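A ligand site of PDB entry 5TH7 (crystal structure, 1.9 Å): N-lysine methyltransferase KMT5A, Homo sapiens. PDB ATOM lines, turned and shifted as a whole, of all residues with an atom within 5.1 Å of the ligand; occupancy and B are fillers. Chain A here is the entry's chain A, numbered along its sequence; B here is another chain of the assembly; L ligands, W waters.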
ATOM      1  N   TYR A  54      -9.851  10.719  10.139  1.00  0.00           N
ATOM      2  CA  TYR A  54      -9.551  11.121  11.496  1.00  0.00           C
ATOM      3  C   TYR A  54      -8.221  11.862  11.277  1.00  0.00           C
ATOM      4  O   TYR A  54      -7.142  11.235  11.227  1.00  0.00           O
ATOM      5  CB  TYR A  54      -9.382   9.923  12.437  1.00  0.00           C
ATOM      6  CG  TYR A  54      -9.057  10.375  13.837  1.00  0.00           C
ATOM      7  CD1 TYR A  54     -10.036  10.958  14.643  1.00  0.00           C
ATOM      8  CD2 TYR A  54      -7.778  10.237  14.355  1.00  0.00           C
ATOM      9  CE1 TYR A  54      -9.737  11.399  15.935  1.00  0.00           C
ATOM     10  CE2 TYR A  54      -7.466  10.647  15.659  1.00  0.00           C
ATOM     11  CZ  TYR A  54      -8.454  11.221  16.444  1.00  0.00           C
ATOM     12  OH  TYR A  54      -8.148  11.641  17.712  1.00  0.00           O
ATOM     13  N   THR A  77      -9.318  14.683  30.719  1.00  0.00           N
ATOM     14  CA  THR A  77     -10.113  15.323  29.665  1.00  0.00           C
ATOM     15  C   THR A  77     -10.051  14.550  28.322  1.00  0.00           C
ATOM     16  O   THR A  77     -10.601  14.999  27.322  1.00  0.00           O
ATOM     17  CB  THR A  77      -9.732  16.813  29.507  1.00  0.00           C
ATOM     18  OG1 THR A  77      -8.366  16.893  29.086  1.00  0.00           O
ATOM     19  CG2 THR A  77      -9.959  17.617  30.817  1.00  0.00           C
ATOM     20  N   GLY A  78      -9.387  13.407  28.318  1.00  0.00           N
ATOM     21  CA  GLY A  78      -9.341  12.593  27.111  1.00  0.00           C
ATOM     22  C   GLY A  78      -8.151  12.837  26.222  1.00  0.00           C
ATOM     23  O   GLY A  78      -7.498  13.878  26.285  1.00  0.00           O
ATOM     24  N   CYS A  79      -7.867  11.866  25.398  1.00  0.00           N
ATOM     25  CA  CYS A  79      -6.692  11.910  24.554  1.00  0.00           C
ATOM     26  C   CYS A  79      -7.069  11.820  23.090  1.00  0.00           C
ATOM     27  O   CYS A  79      -7.836  10.945  22.753  1.00  0.00           O
ATOM     28  CB  CYS A  79      -5.731  10.802  24.952  1.00  0.00           C
ATOM     29  SG  CYS A  79      -4.143  10.873  24.100  1.00  0.00           S
ATOM     30  N   TYR A  80      -6.454  12.656  22.226  1.00  0.00           N
ATOM     31  CA  TYR A  80      -6.694  12.624  20.784  1.00  0.00           C
ATOM     32  C   TYR A  80      -5.635  11.883  19.999  1.00  0.00           C
ATOM     33  O   TYR A  80      -5.724  11.774  18.780  1.00  0.00           O
ATOM     34  CB  TYR A  80      -6.819  14.060  20.228  1.00  0.00           C
ATOM     35  CG  TYR A  80      -8.133  14.698  20.587  1.00  0.00           C
ATOM     36  CD1 TYR A  80      -9.287  14.415  19.848  1.00  0.00           C
ATOM     37  CD2 TYR A  80      -8.238  15.534  21.691  1.00  0.00           C
ATOM     38  CE1 TYR A  80     -10.515  14.982  20.192  1.00  0.00           C
ATOM     39  CE2 TYR A  80      -9.468  16.094  22.058  1.00  0.00           C
ATOM     40  CZ  TYR A  80     -10.600  15.830  21.296  1.00  0.00           C
ATOM     41  OH  TYR A  80     -11.790  16.409  21.655  1.00  0.00           O
ATOM     42  N   MET A  81      -4.654  11.306  20.701  1.00  0.00           N
ATOM     43  CA  MET A  81      -3.562  10.556  20.074  1.00  0.00           C
ATOM     44  C   MET A  81      -3.937   9.093  19.970  1.00  0.00           C
ATOM     45  O   MET A  81      -4.135   8.417  20.989  1.00  0.00           O
ATOM     46  CB  MET A  81      -2.297  10.745  20.917  1.00  0.00           C
ATOM     47  CG  MET A  81      -2.025  12.230  21.195  1.00  0.00           C
ATOM     48  SD  MET A  81      -0.562  12.476  22.158  1.00  0.00           S
ATOM     49  CE  MET A  81       0.764  12.081  20.933  1.00  0.00           C
ATOM     50  N   TYR A  82      -4.084   8.617  18.709  1.00  0.00           N
ATOM     51  CA  TYR A  82      -4.480   7.243  18.383  1.00  0.00           C
ATOM     52  C   TYR A  82      -3.284   6.473  17.837  1.00  0.00           C
ATOM     53  O   TYR A  82      -2.668   6.889  16.854  1.00  0.00           O
ATOM     54  CB  TYR A  82      -5.613   7.260  17.326  1.00  0.00           C
ATOM     55  CG  TYR A  82      -6.085   5.875  16.925  1.00  0.00           C
ATOM     56  CD1 TYR A  82      -7.015   5.175  17.704  1.00  0.00           C
ATOM     57  CD2 TYR A  82      -5.570   5.235  15.795  1.00  0.00           C
ATOM     58  CE1 TYR A  82      -7.430   3.893  17.347  1.00  0.00           C
ATOM     59  CE2 TYR A  82      -5.960   3.938  15.448  1.00  0.00           C
ATOM     60  CZ  TYR A  82      -6.893   3.275  16.227  1.00  0.00           C
ATOM     61  OH  TYR A  82      -7.285   2.016  15.879  1.00  0.00           O
ATOM     62  N   GLY A 103     -13.607  14.972  11.714  1.00  0.00           N
ATOM     63  CA  GLY A 103     -13.330  13.594  12.124  1.00  0.00           C
ATOM     64  C   GLY A 103     -13.155  13.437  13.630  1.00  0.00           C
ATOM     65  O   GLY A 103     -13.782  12.571  14.255  1.00  0.00           O
ATOM     66  N   ARG A 104     -12.383  14.353  14.242  1.00  0.00           N
ATOM     67  CA  ARG A 104     -12.095  14.304  15.687  1.00  0.00           C
ATOM     68  C   ARG A 104     -13.310  14.713  16.549  1.00  0.00           C
ATOM     69  O   ARG A 104     -13.249  14.585  17.757  1.00  0.00           O
ATOM     70  CB  ARG A 104     -10.887  15.197  15.993  1.00  0.00           C
ATOM     71  CG  ARG A 104     -11.148  16.680  15.704  1.00  0.00           C
ATOM     72  CD  ARG A 104      -9.908  17.540  15.781  1.00  0.00           C
ATOM     73  NE  ARG A 104      -9.334  17.551  17.119  1.00  0.00           N
ATOM     74  CZ  ARG A 104      -9.705  18.375  18.096  1.00  0.00           C
ATOM     75  NH1 ARG A 104     -10.693  19.242  17.902  1.00  0.00           N
ATOM     76  NH2 ARG A 104      -9.097  18.338  19.274  1.00  0.00           N
ATOM     77  N   LEU A 105     -14.369  15.269  15.922  1.00  0.00           N
ATOM     78  CA  LEU A 105     -15.612  15.716  16.596  1.00  0.00           C
ATOM     79  C   LEU A 105     -16.705  14.618  16.630  1.00  0.00           C
ATOM     80  O   LEU A 105     -17.698  14.773  17.346  1.00  0.00           O
ATOM     81  CB  LEU A 105     -16.160  16.991  15.927  1.00  0.00           C
ATOM     82  CG  LEU A 105     -15.256  18.267  15.929  1.00  0.00           C
ATOM     83  CD1 LEU A 105     -16.013  19.460  15.389  1.00  0.00           C
ATOM     84  CD2 LEU A 105     -14.780  18.644  17.330  1.00  0.00           C
ATOM     85  N   ILE A 106     -16.536  13.542  15.812  1.00  0.00           N
ATOM     86  CA  ILE A 106     -17.495  12.446  15.725  1.00  0.00           C
ATOM     87  C   ILE A 106     -17.436  11.721  17.056  1.00  0.00           C
ATOM     88  O   ILE A 106     -16.340  11.294  17.503  1.00  0.00           O
ATOM     89  CB  ILE A 106     -17.244  11.540  14.481  1.00  0.00           C
ATOM     90  CG1 ILE A 106     -17.539  12.316  13.171  1.00  0.00           C
ATOM     91  CG2 ILE A 106     -18.059  10.215  14.554  1.00  0.00           C
ATOM     92  CD1 ILE A 106     -17.219  11.600  11.822  1.00  0.00           C
ATOM     93  N   ASN A 107     -18.609  11.622  17.714  1.00  0.00           N
ATOM     94  CA  ASN A 107     -18.681  10.968  19.018  1.00  0.00           C
ATOM     95  C   ASN A 107     -18.527   9.472  18.927  1.00  0.00           C
ATOM     96  O   ASN A 107     -18.751   8.862  17.881  1.00  0.00           O
ATOM     97  CB  ASN A 107     -19.969  11.364  19.794  1.00  0.00           C
ATOM     98  CG  ASN A 107     -19.966  12.792  20.267  1.00  0.00           C
ATOM     99  OD1 ASN A 107     -18.978  13.312  20.817  1.00  0.00           O
ATOM    100  ND2 ASN A 107     -21.087  13.471  20.090  1.00  0.00           N
ATOM    101  N   THR A 116     -13.335   2.282  11.596  1.00  0.00           N
ATOM    102  CA  THR A 116     -12.051   2.759  11.115  1.00  0.00           C
ATOM    103  C   THR A 116     -11.427   1.768  10.144  1.00  0.00           C
ATOM    104  O   THR A 116     -11.624   0.562  10.267  1.00  0.00           O
ATOM    105  CB  THR A 116     -11.106   3.019  12.297  1.00  0.00           C
ATOM    106  OG1 THR A 116     -10.727   1.753  12.843  1.00  0.00           O
ATOM    107  CG2 THR A 116     -11.747   3.870  13.380  1.00  0.00           C
ATOM    108  N   LEU A 127      -5.831   7.302   8.682  1.00  0.00           N
ATOM    109  CA  LEU A 127      -6.879   6.631   9.460  1.00  0.00           C
ATOM    110  C   LEU A 127      -8.222   7.239   9.046  1.00  0.00           C
ATOM    111  O   LEU A 127      -8.462   8.415   9.277  1.00  0.00           O
ATOM    112  CB  LEU A 127      -6.602   6.805  10.964  1.00  0.00           C
ATOM    113  CG  LEU A 127      -7.629   6.211  11.937  1.00  0.00           C
ATOM    114  CD1 LEU A 127      -7.690   4.679  11.865  1.00  0.00           C
ATOM    115  CD2 LEU A 127      -7.295   6.683  13.344  1.00  0.00           C
ATOM    116  N   LEU A 129     -12.648   7.034   8.468  1.00  0.00           N
ATOM    117  CA  LEU A 129     -13.917   6.500   8.948  1.00  0.00           C
ATOM    118  C   LEU A 129     -14.732   6.148   7.735  1.00  0.00           C
ATOM    119  O   LEU A 129     -14.840   6.960   6.826  1.00  0.00           O
ATOM    120  CB  LEU A 129     -14.658   7.497   9.851  1.00  0.00           C
ATOM    121  CG  LEU A 129     -14.110   7.634  11.263  1.00  0.00           C
ATOM    122  CD1 LEU A 129     -14.863   8.700  12.016  1.00  0.00           C
ATOM    123  CD2 LEU A 129     -14.251   6.315  12.058  1.00  0.00           C
ATOM    124  N   TYR A 143     -18.731   6.775  15.928  1.00  0.00           N
ATOM    125  CA  TYR A 143     -17.737   5.758  15.583  1.00  0.00           C
ATOM    126  C   TYR A 143     -17.602   4.729  16.689  1.00  0.00           C
ATOM    127  O   TYR A 143     -17.877   4.999  17.860  1.00  0.00           O
ATOM    128  CB  TYR A 143     -16.340   6.393  15.280  1.00  0.00           C
ATOM    129  CG  TYR A 143     -15.515   6.719  16.524  1.00  0.00           C
ATOM    130  CD1 TYR A 143     -15.687   7.910  17.211  1.00  0.00           C
ATOM    131  CD2 TYR A 143     -14.565   5.816  17.018  1.00  0.00           C
ATOM    132  CE1 TYR A 143     -14.909   8.234  18.318  1.00  0.00           C
ATOM    133  CE2 TYR A 143     -13.856   6.087  18.190  1.00  0.00           C
ATOM    134  CZ  TYR A 143     -14.028   7.296  18.840  1.00  0.00           C
ATOM    135  OH  TYR A 143     -13.265   7.627  19.931  1.00  0.00           O
ATOM    136  N   TYR A 145     -14.490   1.570  17.582  1.00  0.00           N
ATOM    137  CA  TYR A 145     -13.174   1.050  17.211  1.00  0.00           C
ATOM    138  C   TYR A 145     -13.266  -0.346  16.572  1.00  0.00           C
ATOM    139  O   TYR A 145     -12.304  -0.760  15.915  1.00  0.00           O
ATOM    140  CB  TYR A 145     -12.225   1.001  18.441  1.00  0.00           C
ATOM    141  CG  TYR A 145     -12.022   2.313  19.170  1.00  0.00           C
ATOM    142  CD1 TYR A 145     -11.010   3.180  18.794  1.00  0.00           C
ATOM    143  CD2 TYR A 145     -12.764   2.621  20.308  1.00  0.00           C
ATOM    144  CE1 TYR A 145     -10.794   4.368  19.488  1.00  0.00           C
ATOM    145  CE2 TYR A 145     -12.570   3.811  20.996  1.00  0.00           C
ATOM    146  CZ  TYR A 145     -11.577   4.685  20.583  1.00  0.00           C
ATOM    147  OH  TYR A 145     -11.372   5.867  21.265  1.00  0.00           O
ATOM    148  N   GLU B  68      -9.087  -1.572  23.546  1.00  0.00           N
ATOM    149  CA  GLU B  68      -9.618  -0.222  23.272  1.00  0.00           C
ATOM    150  C   GLU B  68     -10.989  -0.375  22.598  1.00  0.00           C
ATOM    151  O   GLU B  68     -11.930   0.311  22.988  1.00  0.00           O
ATOM    152  CB  GLU B  68      -8.609   0.534  22.408  1.00  0.00           C
ATOM    153  CG  GLU B  68      -9.051   1.831  21.786  1.00  0.00           C
ATOM    154  CD  GLU B  68      -7.890   2.484  21.068  1.00  0.00           C
ATOM    155  OE1 GLU B  68      -7.479   1.950  20.024  1.00  0.00           O
ATOM    156  OE2 GLU B  68      -7.400   3.542  21.548  1.00  0.00           O
ATOM    157  N   GLN B  73     -15.345   2.765  25.715  1.00  0.00           N
ATOM    158  CA  GLN B  73     -15.602   3.868  26.644  1.00  0.00           C
ATOM    159  C   GLN B  73     -15.694   5.202  25.967  1.00  0.00           C
ATOM    160  O   GLN B  73     -15.223   5.375  24.823  1.00  0.00           O
ATOM    161  CB  GLN B  73     -14.567   3.905  27.783  1.00  0.00           C
ATOM    162  CG  GLN B  73     -13.123   3.817  27.310  1.00  0.00           C
ATOM    163  CD  GLN B  73     -12.133   3.465  28.404  1.00  0.00           C
ATOM    164  OE1 GLN B  73     -12.470   3.355  29.589  1.00  0.00           O
ATOM    165  NE2 GLN B  73     -10.896   3.248  28.012  1.00  0.00           N
ATOM    166  N   PRO B  75     -14.297   8.531  25.094  1.00  0.00           N
ATOM    167  CA  PRO B  75     -12.914   9.043  25.176  1.00  0.00           C
ATOM    168  C   PRO B  75     -12.739  10.328  26.003  1.00  0.00           C
ATOM    169  O   PRO B  75     -11.619  10.613  26.384  1.00  0.00           O
ATOM    170  CB  PRO B  75     -12.532   9.248  23.707  1.00  0.00           C
ATOM    171  CG  PRO B  75     -13.836   9.510  23.031  1.00  0.00           C
ATOM    172  CD  PRO B  75     -14.808   8.616  23.710  1.00  0.00           C
ATOM    173  N   SER B  76     -13.819  11.056  26.309  1.00  0.00           N
ATOM    174  CA  SER B  76     -13.739  12.319  27.059  1.00  0.00           C
ATOM    175  C   SER B  76     -13.330  12.149  28.543  1.00  0.00           C
ATOM    176  O   SER B  76     -12.897  13.121  29.165  1.00  0.00           O
ATOM    177  CB  SER B  76     -15.054  13.100  26.940  1.00  0.00           C
ATOM    178  OG  SER B  76     -16.139  12.413  27.534  1.00  0.00           O
ATOM    179  N   GLY B  78     -10.881  10.176  29.567  1.00  0.00           N
ATOM    180  CA  GLY B  78      -9.464   9.863  29.707  1.00  0.00           C
ATOM    181  C   GLY B  78      -9.144   8.418  29.487  1.00  0.00           C
ATOM    182  O   GLY B  78     -10.003   7.547  29.555  1.00  0.00           O
ATOM    183  N   CYS B  79      -7.880   8.150  29.264  1.00  0.00           N
ATOM    184  CA  CYS B  79      -7.431   6.826  28.896  1.00  0.00           C
ATOM    185  C   CYS B  79      -6.334   6.366  29.832  1.00  0.00           C
ATOM    186  O   CYS B  79      -5.414   7.124  30.065  1.00  0.00           O
ATOM    187  CB  CYS B  79      -6.940   6.876  27.442  1.00  0.00           C
ATOM    188  SG  CYS B  79      -6.475   5.263  26.770  1.00  0.00           S
ATOM    189  N   TYR B  80      -6.369   5.078  30.268  1.00  0.00           N
ATOM    190  CA  TYR B  80      -5.351   4.493  31.150  1.00  0.00           C
ATOM    191  C   TYR B  80      -4.333   3.628  30.404  1.00  0.00           C
ATOM    192  O   TYR B  80      -3.489   3.011  31.047  1.00  0.00           O
ATOM    193  CB  TYR B  80      -6.019   3.697  32.277  1.00  0.00           C
ATOM    194  CG  TYR B  80      -6.668   4.571  33.321  1.00  0.00           C
ATOM    195  CD1 TYR B  80      -5.920   5.111  34.368  1.00  0.00           C
ATOM    196  CD2 TYR B  80      -8.022   4.898  33.231  1.00  0.00           C
ATOM    197  CE1 TYR B  80      -6.520   5.916  35.336  1.00  0.00           C
ATOM    198  CE2 TYR B  80      -8.629   5.742  34.186  1.00  0.00           C
ATOM    199  CZ  TYR B  80      -7.872   6.240  35.237  1.00  0.00           C
ATOM    200  OH  TYR B  80      -8.445   7.080  36.157  1.00  0.00           O
ATOM    201  N   MET B  81      -4.429   3.578  29.070  1.00  0.00           N
ATOM    202  CA  MET B  81      -3.548   2.762  28.217  1.00  0.00           C
ATOM    203  C   MET B  81      -2.376   3.613  27.720  1.00  0.00           C
ATOM    204  O   MET B  81      -2.587   4.612  27.021  1.00  0.00           O
ATOM    205  CB  MET B  81      -4.355   2.161  27.069  1.00  0.00           C
ATOM    206  CG  MET B  81      -5.571   1.368  27.519  1.00  0.00           C
ATOM    207  SD  MET B  81      -6.567   0.814  26.105  1.00  0.00           S
ATOM    208  CE  MET B  81      -5.612  -0.594  25.570  1.00  0.00           C
HETATM  209  C1  LIG L   1     -11.895  10.601  19.147  1.00  0.00           C
HETATM  210  C2  LIG L   1     -10.834  10.528  20.078  1.00  0.00           C
HETATM  211  C3  LIG L   1      -9.774   9.592  19.754  1.00  0.00           C
HETATM  212  N1  LIG L   1      -9.833   8.842  18.666  1.00  0.00           N
HETATM  213  N2  LIG L   1     -11.923   9.846  18.003  1.00  0.00           N
HETATM  214  C4  LIG L   1      -9.948   7.094  16.607  1.00  0.00           C
HETATM  215  C5  LIG L   1     -10.416   6.351  15.379  1.00  0.00           C
HETATM  216  C6  LIG L   1     -11.360   7.264  14.660  1.00  0.00           C
HETATM  217  C7  LIG L   1     -11.990   8.086  15.766  1.00  0.00           C
HETATM  218  N3  LIG L   1     -10.920   8.175  16.768  1.00  0.00           N
HETATM  219  C8  LIG L   1     -10.895   8.982  17.843  1.00  0.00           C
HETATM  220  C9  LIG L   1     -12.976  11.470  19.422  1.00  0.00           C
HETATM  221  C10 LIG L   1     -13.012  12.209  20.578  1.00  0.00           C
HETATM  222  O1  LIG L   1     -14.060  13.002  20.968  1.00  0.00           O
HETATM  223  C11 LIG L   1     -15.181  13.145  20.078  1.00  0.00           C
HETATM  224  C12 LIG L   1     -11.944  12.141  21.499  1.00  0.00           C
HETATM  225  O2  LIG L   1     -12.100  12.916  22.610  1.00  0.00           O
HETATM  226  C13 LIG L   1     -11.011  13.004  23.531  1.00  0.00           C
HETATM  227  C14 LIG L   1     -10.880  11.325  21.258  1.00  0.00           C
HETATM  228  N4  LIG L   1      -8.704   9.429  20.618  1.00  0.00           N
HETATM  229  C15 LIG L   1      -7.594   8.529  20.348  1.00  0.00           C
HETATM  230  C16 LIG L   1      -7.793   7.176  20.981  1.00  0.00           C
HETATM  231  C17 LIG L   1      -7.918   7.253  22.484  1.00  0.00           C
HETATM  232  N5  LIG L   1      -8.121   5.964  23.131  1.00  0.00           N
HETATM  233  C18 LIG L   1      -8.645   5.875  24.356  1.00  0.00           C
HETATM  234  O3  LIG L   1      -9.086   6.867  24.950  1.00  0.00           O
HETATM  235  C19 LIG L   1      -8.617   4.503  24.978  1.00  0.00           C
HETATM  236  C20 LIG L   1      -8.094   4.516  26.421  1.00  0.00           C
HETATM  237  O   HOH W   1      -8.505   3.405  29.554  1.00  0.00           O
HETATM  238  O   HOH W   2      -9.279   9.462  25.782  1.00  0.00           O
HETATM  239  O   HOH W   3     -13.681  16.268  19.861  1.00  0.00           O
HETATM  240  O   HOH W   4     -13.885  10.839  16.349  1.00  0.00           O
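Gly 78 of chain A touches the ligand (C to C13, 3.9 Å).
CE1 of Tyr 80 of chain A touches C12 of the ligand, at 3.4 Å.
Met 81 of chain A touches the ligand (O to C15, 3.5 Å).
CD1 of Tyr 82 touches C4 of the ligand (3.7 Å).
O of Arg 104 touches C11 of the ligand, 3.3 Å away.
O of Ile 106 touches C11 of the ligand (3.4 Å).
Asn 107 touches the ligand.
CG2 of Thr 116 touches C5 of the ligand, 3.5 Å away.
Leu 127 touches the ligand.
OH of Tyr 145 touches N5 of the ligand, at 3.7 Å.
Gln 73 of chain B touches the ligand (NE2 to C20, 3.5 Å).
Pro 75 of chain B touches the ligand.
Hydrophobic or aromatic side chains that line the ligand: Tyr 54, Tyr 80 of chain A, Tyr 82, Leu 127, Tyr 143 and Pro 75 of chain B.
Water W2 lies within hydrogen-bond range of O of Pro 75 of chain B (2.7 Å), O3 of the ligand (2.7 Å) and N of Cys 79 of chain A (2.8 Å).
Water W1 bridges the backbone NH of Tyr 80 of chain B (2.8 Å) and the side-chain amide nitrogen of Gln 73 of chain B (2.8 Å).
Water W3 lies within hydrogen-bond range of OH of Tyr 80 of chain A, O of Arg 104 and O1 of the ligand.
SG of Cys 79 of chain B is bonded to C20 of the ligand (1.8 Å).
N4 of the ligand is in hydrogen-bond range of O of Cys 79 of chain A (2.8 Å).
N5 of the ligand lies within hydrogen-bond range of OE2 of Glu 68 of chain B (3.0 Å).
OH of Tyr 143 is in hydrogen-bond range of N2 of the ligand (3.2 Å).
N1 of the ligand lies close to OH of Tyr 54 (3.4 Å).
The side-chain sulfur (SG) of Cys 79 of chain B sits close to the backbone NH (N) of Met 81 of chain B, at 3.5 Å.
N of Met 81 of chain A sits close to SG of Cys 79 of chain A (3.5 Å).
The side-chain hydroxyl (OH) of Tyr 143 sits at hydrogen-bond distance from the side-chain hydroxyl (OH) of Tyr 145, 2.9 Å away.
N of Tyr 143 is in hydrogen-bond range of O of Asn 107.
O of Tyr 80 of chain A sits at hydrogen-bond distance from OH of Tyr 54, 2.7 Å away.
The backbone NH (N) of Tyr 54 lies within hydrogen-bond range of the backbone carbonyl oxygen (O) of Leu 127 (2.8 Å).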
